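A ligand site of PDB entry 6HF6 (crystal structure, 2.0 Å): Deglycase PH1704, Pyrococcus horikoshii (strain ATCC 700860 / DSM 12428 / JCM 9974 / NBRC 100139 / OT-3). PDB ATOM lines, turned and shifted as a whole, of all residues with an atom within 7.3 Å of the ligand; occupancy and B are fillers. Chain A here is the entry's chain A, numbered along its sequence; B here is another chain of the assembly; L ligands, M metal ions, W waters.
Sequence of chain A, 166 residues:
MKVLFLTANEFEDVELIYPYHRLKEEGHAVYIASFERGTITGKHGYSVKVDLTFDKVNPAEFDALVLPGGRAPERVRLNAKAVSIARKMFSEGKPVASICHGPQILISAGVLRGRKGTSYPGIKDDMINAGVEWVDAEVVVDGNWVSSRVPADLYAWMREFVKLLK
Ala 8 touches the ligand (CB to O1, 3.0 Å). OG of Ser 34 touches C1 of the ligand, 3.99 Å away. Phe 35 touches the ligand (CZ to C20, 3.6 Å). OE1 of Glu 36 touches C15 of the ligand (3.6 Å). CG2 of Ile 40 touches C1 of the ligand, 3.8 Å away. Hydrophobic or aromatic side chains that line the ligand: Ala 8, Phe 35 and Ile 40. Seven residues have an atom within 4 Å of the ligand: Ala 8, Asn 9, Ser 34, Phe 35, Glu 36, Ile 40 and Arg 75.
The side-chain hydroxyl (OG) of Ser 34 sits at hydrogen-bond distance from the backbone carbonyl oxygen (O) of Thr 7. The backbone NH (N) of Phe 54 lies within hydrogen-bond range of the backbone carbonyl oxygen (O) of Ser 34. OD1 of Asn 9 is in hydrogen-bond range of N of Thr 41 (2.9 Å).
An oxygen (O1) of the ligand is in hydrogen-bond range of the backbone NH of Asn 9 (2.7 Å). The guanidinium group (NH1) of Arg 75 lies within salt-bridge range of an oxygen (O2) of the ligand (2.7 Å).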
ATOM      1  N   THR A   7      20.035  20.492   7.428  1.00  0.00           N
ATOM      2  CA  THR A   7      19.948  19.113   7.912  1.00  0.00           C
ATOM      3  C   THR A   7      18.523  18.560   7.772  1.00  0.00           C
ATOM      4  O   THR A   7      17.648  19.215   7.201  1.00  0.00           O
ATOM      5  CB  THR A   7      20.491  19.079   9.379  1.00  0.00           C
ATOM      6  OG1 THR A   7      20.581  17.728   9.834  1.00  0.00           O
ATOM      7  CG2 THR A   7      19.671  19.919  10.333  1.00  0.00           C
ATOM      8  N   ALA A   8      18.305  17.358   8.276  1.00  0.00           N
ATOM      9  CA  ALA A   8      17.018  16.679   8.168  1.00  0.00           C
ATOM     10  C   ALA A   8      16.973  15.510   9.119  1.00  0.00           C
ATOM     11  O   ALA A   8      17.928  15.316   9.863  1.00  0.00           O
ATOM     12  CB  ALA A   8      16.821  16.194   6.720  1.00  0.00           C
ATOM     13  N   ASN A   9      15.918  14.683   9.056  1.00  0.00           N
ATOM     14  CA  ASN A   9      15.839  13.499   9.918  1.00  0.00           C
ATOM     15  C   ASN A   9      17.013  12.573   9.613  1.00  0.00           C
ATOM     16  O   ASN A   9      17.530  12.556   8.504  1.00  0.00           O
ATOM     17  CB  ASN A   9      14.510  12.727   9.727  1.00  0.00           C
ATOM     18  CG  ASN A   9      13.343  13.433  10.331  1.00  0.00           C
ATOM     19  OD1 ASN A   9      13.403  13.913  11.453  1.00  0.00           O
ATOM     20  ND2 ASN A   9      12.236  13.518   9.623  1.00  0.00           N
ATOM     21  N   GLU A  10      17.445  11.816  10.635  1.00  0.00           N
ATOM     22  CA  GLU A  10      18.569  10.880  10.552  1.00  0.00           C
ATOM     23  C   GLU A  10      19.917  11.554  10.422  1.00  0.00           C
ATOM     24  O   GLU A  10      20.874  10.949   9.926  1.00  0.00           O
ATOM     25  CB  GLU A  10      18.373   9.855   9.442  1.00  0.00           C
ATOM     26  CG  GLU A  10      16.992   9.217   9.452  1.00  0.00           C
ATOM     27  CD  GLU A  10      17.001   7.840  10.048  1.00  0.00           C
ATOM     28  OE1 GLU A  10      16.933   6.858   9.273  1.00  0.00           O
ATOM     29  OE2 GLU A  10      17.128   7.737  11.292  1.00  0.00           O
ATOM     30  N   SER A  34      15.464  23.007   7.787  1.00  0.00           N
ATOM     31  CA  SER A  34      15.107  21.686   7.257  1.00  0.00           C
ATOM     32  C   SER A  34      13.884  21.770   6.336  1.00  0.00           C
ATOM     33  O   SER A  34      13.518  22.861   5.929  1.00  0.00           O
ATOM     34  CB  SER A  34      14.913  20.677   8.387  1.00  0.00           C
ATOM     35  OG  SER A  34      14.964  19.363   7.836  1.00  0.00           O
ATOM     36  N   PHE A  35      13.314  20.618   5.939  1.00  0.00           N
ATOM     37  CA  PHE A  35      12.205  20.571   4.972  1.00  0.00           C
ATOM     38  C   PHE A  35      10.944  21.240   5.476  1.00  0.00           C
ATOM     39  O   PHE A  35      10.250  21.899   4.701  1.00  0.00           O
ATOM     40  CB  PHE A  35      11.873  19.110   4.626  1.00  0.00           C
ATOM     41  CG  PHE A  35      12.967  18.425   3.845  1.00  0.00           C
ATOM     42  CD1 PHE A  35      13.040  18.557   2.472  1.00  0.00           C
ATOM     43  CD2 PHE A  35      13.908  17.628   4.484  1.00  0.00           C
ATOM     44  CE1 PHE A  35      14.020  17.897   1.736  1.00  0.00           C
ATOM     45  CE2 PHE A  35      14.914  16.985   3.745  1.00  0.00           C
ATOM     46  CZ  PHE A  35      14.954  17.128   2.383  1.00  0.00           C
ATOM     47  N   GLU A  36      10.626  21.045   6.751  1.00  0.00           N
ATOM     48  CA  GLU A  36       9.407  21.568   7.361  1.00  0.00           C
ATOM     49  C   GLU A  36       9.653  22.043   8.772  1.00  0.00           C
ATOM     50  O   GLU A  36      10.614  21.613   9.411  1.00  0.00           O
ATOM     51  CB  GLU A  36       8.349  20.453   7.447  1.00  0.00           C
ATOM     52  CG  GLU A  36       8.067  19.764   6.125  1.00  0.00           C
ATOM     53  CD  GLU A  36       6.883  18.826   6.156  1.00  0.00           C
ATOM     54  OE1 GLU A  36       6.499  18.384   7.269  1.00  0.00           O
ATOM     55  OE2 GLU A  36       6.337  18.517   5.081  1.00  0.00           O
ATOM     56  N   ARG A  37       8.730  22.857   9.272  1.00  0.00           N
ATOM     57  CA  ARG A  37       8.768  23.333  10.653  1.00  0.00           C
ATOM     58  C   ARG A  37       8.419  22.174  11.580  1.00  0.00           C
ATOM     59  O   ARG A  37       7.897  21.152  11.136  1.00  0.00           O
ATOM     60  CB  ARG A  37       7.749  24.470  10.869  1.00  0.00           C
ATOM     61  CG  ARG A  37       7.980  25.713  10.001  1.00  0.00           C
ATOM     62  CD  ARG A  37       9.320  26.375  10.250  1.00  0.00           C
ATOM     63  NE  ARG A  37       9.527  26.758  11.651  1.00  0.00           N
ATOM     64  CZ  ARG A  37       9.012  27.835  12.240  1.00  0.00           C
ATOM     65  NH1 ARG A  37       8.229  28.681  11.560  1.00  0.00           N
ATOM     66  NH2 ARG A  37       9.274  28.086  13.514  1.00  0.00           N
ATOM     67  N   GLY A  38       8.718  22.337  12.857  1.00  0.00           N
ATOM     68  CA  GLY A  38       8.459  21.325  13.867  1.00  0.00           C
ATOM     69  C   GLY A  38       9.791  20.783  14.343  1.00  0.00           C
ATOM     70  O   GLY A  38      10.681  21.570  14.641  1.00  0.00           O
ATOM     71  N   THR A  39       9.942  19.462  14.398  1.00  0.00           N
ATOM     72  CA  THR A  39      11.184  18.875  14.888  1.00  0.00           C
ATOM     73  C   THR A  39      11.721  17.840  13.933  1.00  0.00           C
ATOM     74  O   THR A  39      10.967  17.301  13.126  1.00  0.00           O
ATOM     75  CB  THR A  39      10.965  18.202  16.277  1.00  0.00           C
ATOM     76  OG1 THR A  39      10.115  17.078  16.117  1.00  0.00           O
ATOM     77  CG2 THR A  39      10.360  19.157  17.306  1.00  0.00           C
ATOM     78  N   ILE A  40      13.016  17.556  14.063  1.00  0.00           N
ATOM     79  CA  ILE A  40      13.695  16.499  13.310  1.00  0.00           C
ATOM     80  C   ILE A  40      14.375  15.627  14.348  1.00  0.00           C
ATOM     81  O   ILE A  40      14.702  16.115  15.435  1.00  0.00           O
ATOM     82  CB  ILE A  40      14.669  17.034  12.212  1.00  0.00           C
ATOM     83  CG1 ILE A  40      15.601  18.117  12.784  1.00  0.00           C
ATOM     84  CG2 ILE A  40      13.857  17.536  10.980  1.00  0.00           C
ATOM     85  CD1 ILE A  40      16.757  18.527  11.834  1.00  0.00           C
ATOM     86  N   THR A  41      14.588  14.350  14.027  1.00  0.00           N
ATOM     87  CA  THR A  41      15.146  13.366  14.978  1.00  0.00           C
ATOM     88  C   THR A  41      16.400  12.740  14.390  1.00  0.00           C
ATOM     89  O   THR A  41      16.384  12.335  13.230  1.00  0.00           O
ATOM     90  CB  THR A  41      14.046  12.352  15.319  1.00  0.00           C
ATOM     91  OG1 THR A  41      12.912  13.078  15.802  1.00  0.00           O
ATOM     92  CG2 THR A  41      14.489  11.323  16.374  1.00  0.00           C
ATOM     93  N   VAL A  50      13.217  22.731  14.381  1.00  0.00           N
ATOM     94  CA  VAL A  50      13.605  23.337  13.103  1.00  0.00           C
ATOM     95  C   VAL A  50      13.251  24.832  13.244  1.00  0.00           C
ATOM     96  O   VAL A  50      12.124  25.167  13.609  1.00  0.00           O
ATOM     97  CB  VAL A  50      12.863  22.682  11.919  1.00  0.00           C
ATOM     98  CG1 VAL A  50      13.137  23.448  10.620  1.00  0.00           C
ATOM     99  CG2 VAL A  50      13.274  21.211  11.778  1.00  0.00           C
ATOM    100  N   PHE A  54      13.837  25.312   4.275  1.00  0.00           N
ATOM    101  CA  PHE A  54      14.760  25.670   3.195  1.00  0.00           C
ATOM    102  C   PHE A  54      14.176  26.782   2.299  1.00  0.00           C
ATOM    103  O   PHE A  54      14.884  27.717   1.948  1.00  0.00           O
ATOM    104  CB  PHE A  54      15.083  24.455   2.288  1.00  0.00           C
ATOM    105  CG  PHE A  54      15.714  23.278   2.999  1.00  0.00           C
ATOM    106  CD1 PHE A  54      16.786  23.467   3.881  1.00  0.00           C
ATOM    107  CD2 PHE A  54      15.253  21.976   2.774  1.00  0.00           C
ATOM    108  CE1 PHE A  54      17.402  22.380   4.488  1.00  0.00           C
ATOM    109  CE2 PHE A  54      15.891  20.892   3.387  1.00  0.00           C
ATOM    110  CZ  PHE A  54      16.969  21.097   4.217  1.00  0.00           C
ATOM    111  N   ALA A  72      21.040  12.249   6.766  1.00  0.00           N
ATOM    112  CA  ALA A  72      20.319  13.462   6.349  1.00  0.00           C
ATOM    113  C   ALA A  72      20.868  14.089   5.055  1.00  0.00           C
ATOM    114  O   ALA A  72      20.067  14.493   4.221  1.00  0.00           O
ATOM    115  CB  ALA A  72      20.332  14.505   7.469  1.00  0.00           C
ATOM    116  N   GLU A  74      21.972  12.932   2.227  1.00  0.00           N
ATOM    117  CA  GLU A  74      21.419  12.299   1.009  1.00  0.00           C
ATOM    118  C   GLU A  74      19.934  12.703   0.743  1.00  0.00           C
ATOM    119  O   GLU A  74      19.478  12.666  -0.392  1.00  0.00           O
ATOM    120  CB  GLU A  74      21.572  10.761   1.080  1.00  0.00           C
ATOM    121  CG  GLU A  74      22.908  10.358   0.487  1.00  0.00           C
ATOM    122  CD  GLU A  74      23.240   8.890   0.653  1.00  0.00           C
ATOM    123  OE1 GLU A  74      22.277   8.095   0.510  1.00  0.00           O
ATOM    124  OE2 GLU A  74      24.407   8.525   0.925  1.00  0.00           O
ATOM    125  N   ARG A  75      19.198  13.126   1.776  1.00  0.00           N
ATOM    126  CA  ARG A  75      17.833  13.668   1.614  1.00  0.00           C
ATOM    127  C   ARG A  75      17.950  15.155   1.230  1.00  0.00           C
ATOM    128  O   ARG A  75      17.316  15.607   0.289  1.00  0.00           O
ATOM    129  CB  ARG A  75      17.048  13.583   2.940  1.00  0.00           C
ATOM    130  CG  ARG A  75      16.996  12.197   3.593  1.00  0.00           C
ATOM    131  CD  ARG A  75      15.987  12.224   4.748  1.00  0.00           C
ATOM    132  NE  ARG A  75      15.903  10.900   5.380  1.00  0.00           N
ATOM    133  CZ  ARG A  75      14.873  10.454   6.111  1.00  0.00           C
ATOM    134  NH1 ARG A  75      13.836  11.251   6.384  1.00  0.00           N
ATOM    135  NH2 ARG A  75      14.879   9.218   6.580  1.00  0.00           N
ATOM    136  N   VAL A  76      18.780  15.908   1.980  1.00  0.00           N
ATOM    137  CA  VAL A  76      18.962  17.346   1.748  1.00  0.00           C
ATOM    138  C   VAL A  76      19.441  17.645   0.315  1.00  0.00           C
ATOM    139  O   VAL A  76      18.977  18.609  -0.295  1.00  0.00           O
ATOM    140  CB  VAL A  76      19.919  18.006   2.792  1.00  0.00           C
ATOM    141  CG1 VAL A  76      20.170  19.483   2.477  1.00  0.00           C
ATOM    142  CG2 VAL A  76      19.352  17.860   4.217  1.00  0.00           C
ATOM    143  N   LEU A  78      18.786  16.311  -2.453  1.00  0.00           N
ATOM    144  CA  LEU A  78      17.720  16.174  -3.440  1.00  0.00           C
ATOM    145  C   LEU A  78      16.802  17.395  -3.444  1.00  0.00           C
ATOM    146  O   LEU A  78      15.936  17.494  -4.306  1.00  0.00           O
ATOM    147  CB  LEU A  78      16.884  14.910  -3.201  1.00  0.00           C
ATOM    148  CG  LEU A  78      17.632  13.591  -3.449  1.00  0.00           C
ATOM    149  CD1 LEU A  78      16.746  12.401  -3.139  1.00  0.00           C
ATOM    150  CD2 LEU A  78      18.152  13.527  -4.886  1.00  0.00           C
ATOM    151  N   ASN A  79      16.990  18.337  -2.498  1.00  0.00           N
ATOM    152  CA  ASN A  79      16.170  19.555  -2.443  1.00  0.00           C
ATOM    153  C   ASN A  79      16.944  20.646  -3.147  1.00  0.00           C
ATOM    154  O   ASN A  79      18.001  21.050  -2.669  1.00  0.00           O
ATOM    155  CB  ASN A  79      15.883  19.931  -0.978  1.00  0.00           C
ATOM    156  CG  ASN A  79      14.950  21.097  -0.874  1.00  0.00           C
ATOM    157  OD1 ASN A  79      15.394  22.234  -0.870  1.00  0.00           O
ATOM    158  ND2 ASN A  79      13.649  20.845  -0.802  1.00  0.00           N
ATOM    159  N   TYR B 120      19.687   4.580  -6.049  1.00  0.00           N
ATOM    160  CA  TYR B 120      18.943   5.358  -5.075  1.00  0.00           C
ATOM    161  C   TYR B 120      19.080   6.836  -5.530  1.00  0.00           C
ATOM    162  O   TYR B 120      20.203   7.265  -5.813  1.00  0.00           O
ATOM    163  CB  TYR B 120      19.601   5.202  -3.686  1.00  0.00           C
ATOM    164  CG  TYR B 120      18.912   6.005  -2.605  1.00  0.00           C
ATOM    165  CD1 TYR B 120      17.582   5.771  -2.278  1.00  0.00           C
ATOM    166  CD2 TYR B 120      19.602   6.967  -1.879  1.00  0.00           C
ATOM    167  CE1 TYR B 120      16.950   6.505  -1.280  1.00  0.00           C
ATOM    168  CE2 TYR B 120      18.978   7.706  -0.892  1.00  0.00           C
ATOM    169  CZ  TYR B 120      17.649   7.480  -0.596  1.00  0.00           C
ATOM    170  OH  TYR B 120      16.994   8.180   0.391  1.00  0.00           O
HETATM  171  C1  LIG L   1      12.089  16.598   7.721  1.00  0.00           C
HETATM  172  C2  LIG L   1      12.775  13.534   2.319  1.00  0.00           C
HETATM  173  C3  LIG L   1       9.600  15.828   6.807  1.00  0.00           C
HETATM  174  C4  LIG L   1      10.115  16.115   3.336  1.00  0.00           C
HETATM  175  C5  LIG L   1       8.658  16.041   3.899  1.00  0.00           C
HETATM  176  C6  LIG L   1       9.898  14.323   1.632  1.00  0.00           C
HETATM  177  C7  LIG L   1       9.370  12.889   1.786  1.00  0.00           C
HETATM  178  C8  LIG L   1       7.387  13.290   3.180  1.00  0.00           C
HETATM  179  C9  LIG L   1       7.251  14.039   4.507  1.00  0.00           C
HETATM  180  C10 LIG L   1      13.785  13.270   1.408  1.00  0.00           C
HETATM  181  C11 LIG L   1      14.297  12.002   1.275  1.00  0.00           C
HETATM  182  C12 LIG L   1      13.782  10.968   2.030  1.00  0.00           C
HETATM  183  C13 LIG L   1      12.741  11.252   2.921  1.00  0.00           C
HETATM  184  C14 LIG L   1      12.058  10.227   3.806  1.00  0.00           C
HETATM  185  C15 LIG L   1       9.736  16.939   7.635  1.00  0.00           C
HETATM  186  C16 LIG L   1      10.987  17.314   8.077  1.00  0.00           C
HETATM  187  C17 LIG L   1      11.903  15.475   6.892  1.00  0.00           C
HETATM  188  C18 LIG L   1      13.080  14.629   6.456  1.00  0.00           C
HETATM  189  C19 LIG L   1       8.236  15.337   6.263  1.00  0.00           C
HETATM  190  C20 LIG L   1      12.121  14.940   2.529  1.00  0.00           C
HETATM  191  N1  LIG L   1      10.652  14.816   2.799  1.00  0.00           N
HETATM  192  N2  LIG L   1       8.646  12.584   3.038  1.00  0.00           N
HETATM  193  N3  LIG L   1       8.406  14.895   4.857  1.00  0.00           N
HETATM  194  N4  LIG L   1      12.278  12.517   3.030  1.00  0.00           N
HETATM  195  N5  LIG L   1      10.669  15.115   6.449  1.00  0.00           N
HETATM  196  O1  LIG L   1      14.150  14.841   6.984  1.00  0.00           O
HETATM  197  O2  LIG L   1      13.004  13.740   5.566  1.00  0.00           O
HETATM  198  O3  LIG L   1      11.040  10.620   4.440  1.00  0.00           O
HETATM  199  O4  LIG L   1      12.489   9.059   3.895  1.00  0.00           O
HETATM  200 TB1  LIG L   1      10.566  13.006   4.911  1.00  0.00          TB
HETATM  201 TB    TB M   1      16.309   5.330   7.616  1.00  0.00          TB
HETATM  202  O   HOH W   1      10.123  18.802  10.682  1.00  0.00           O
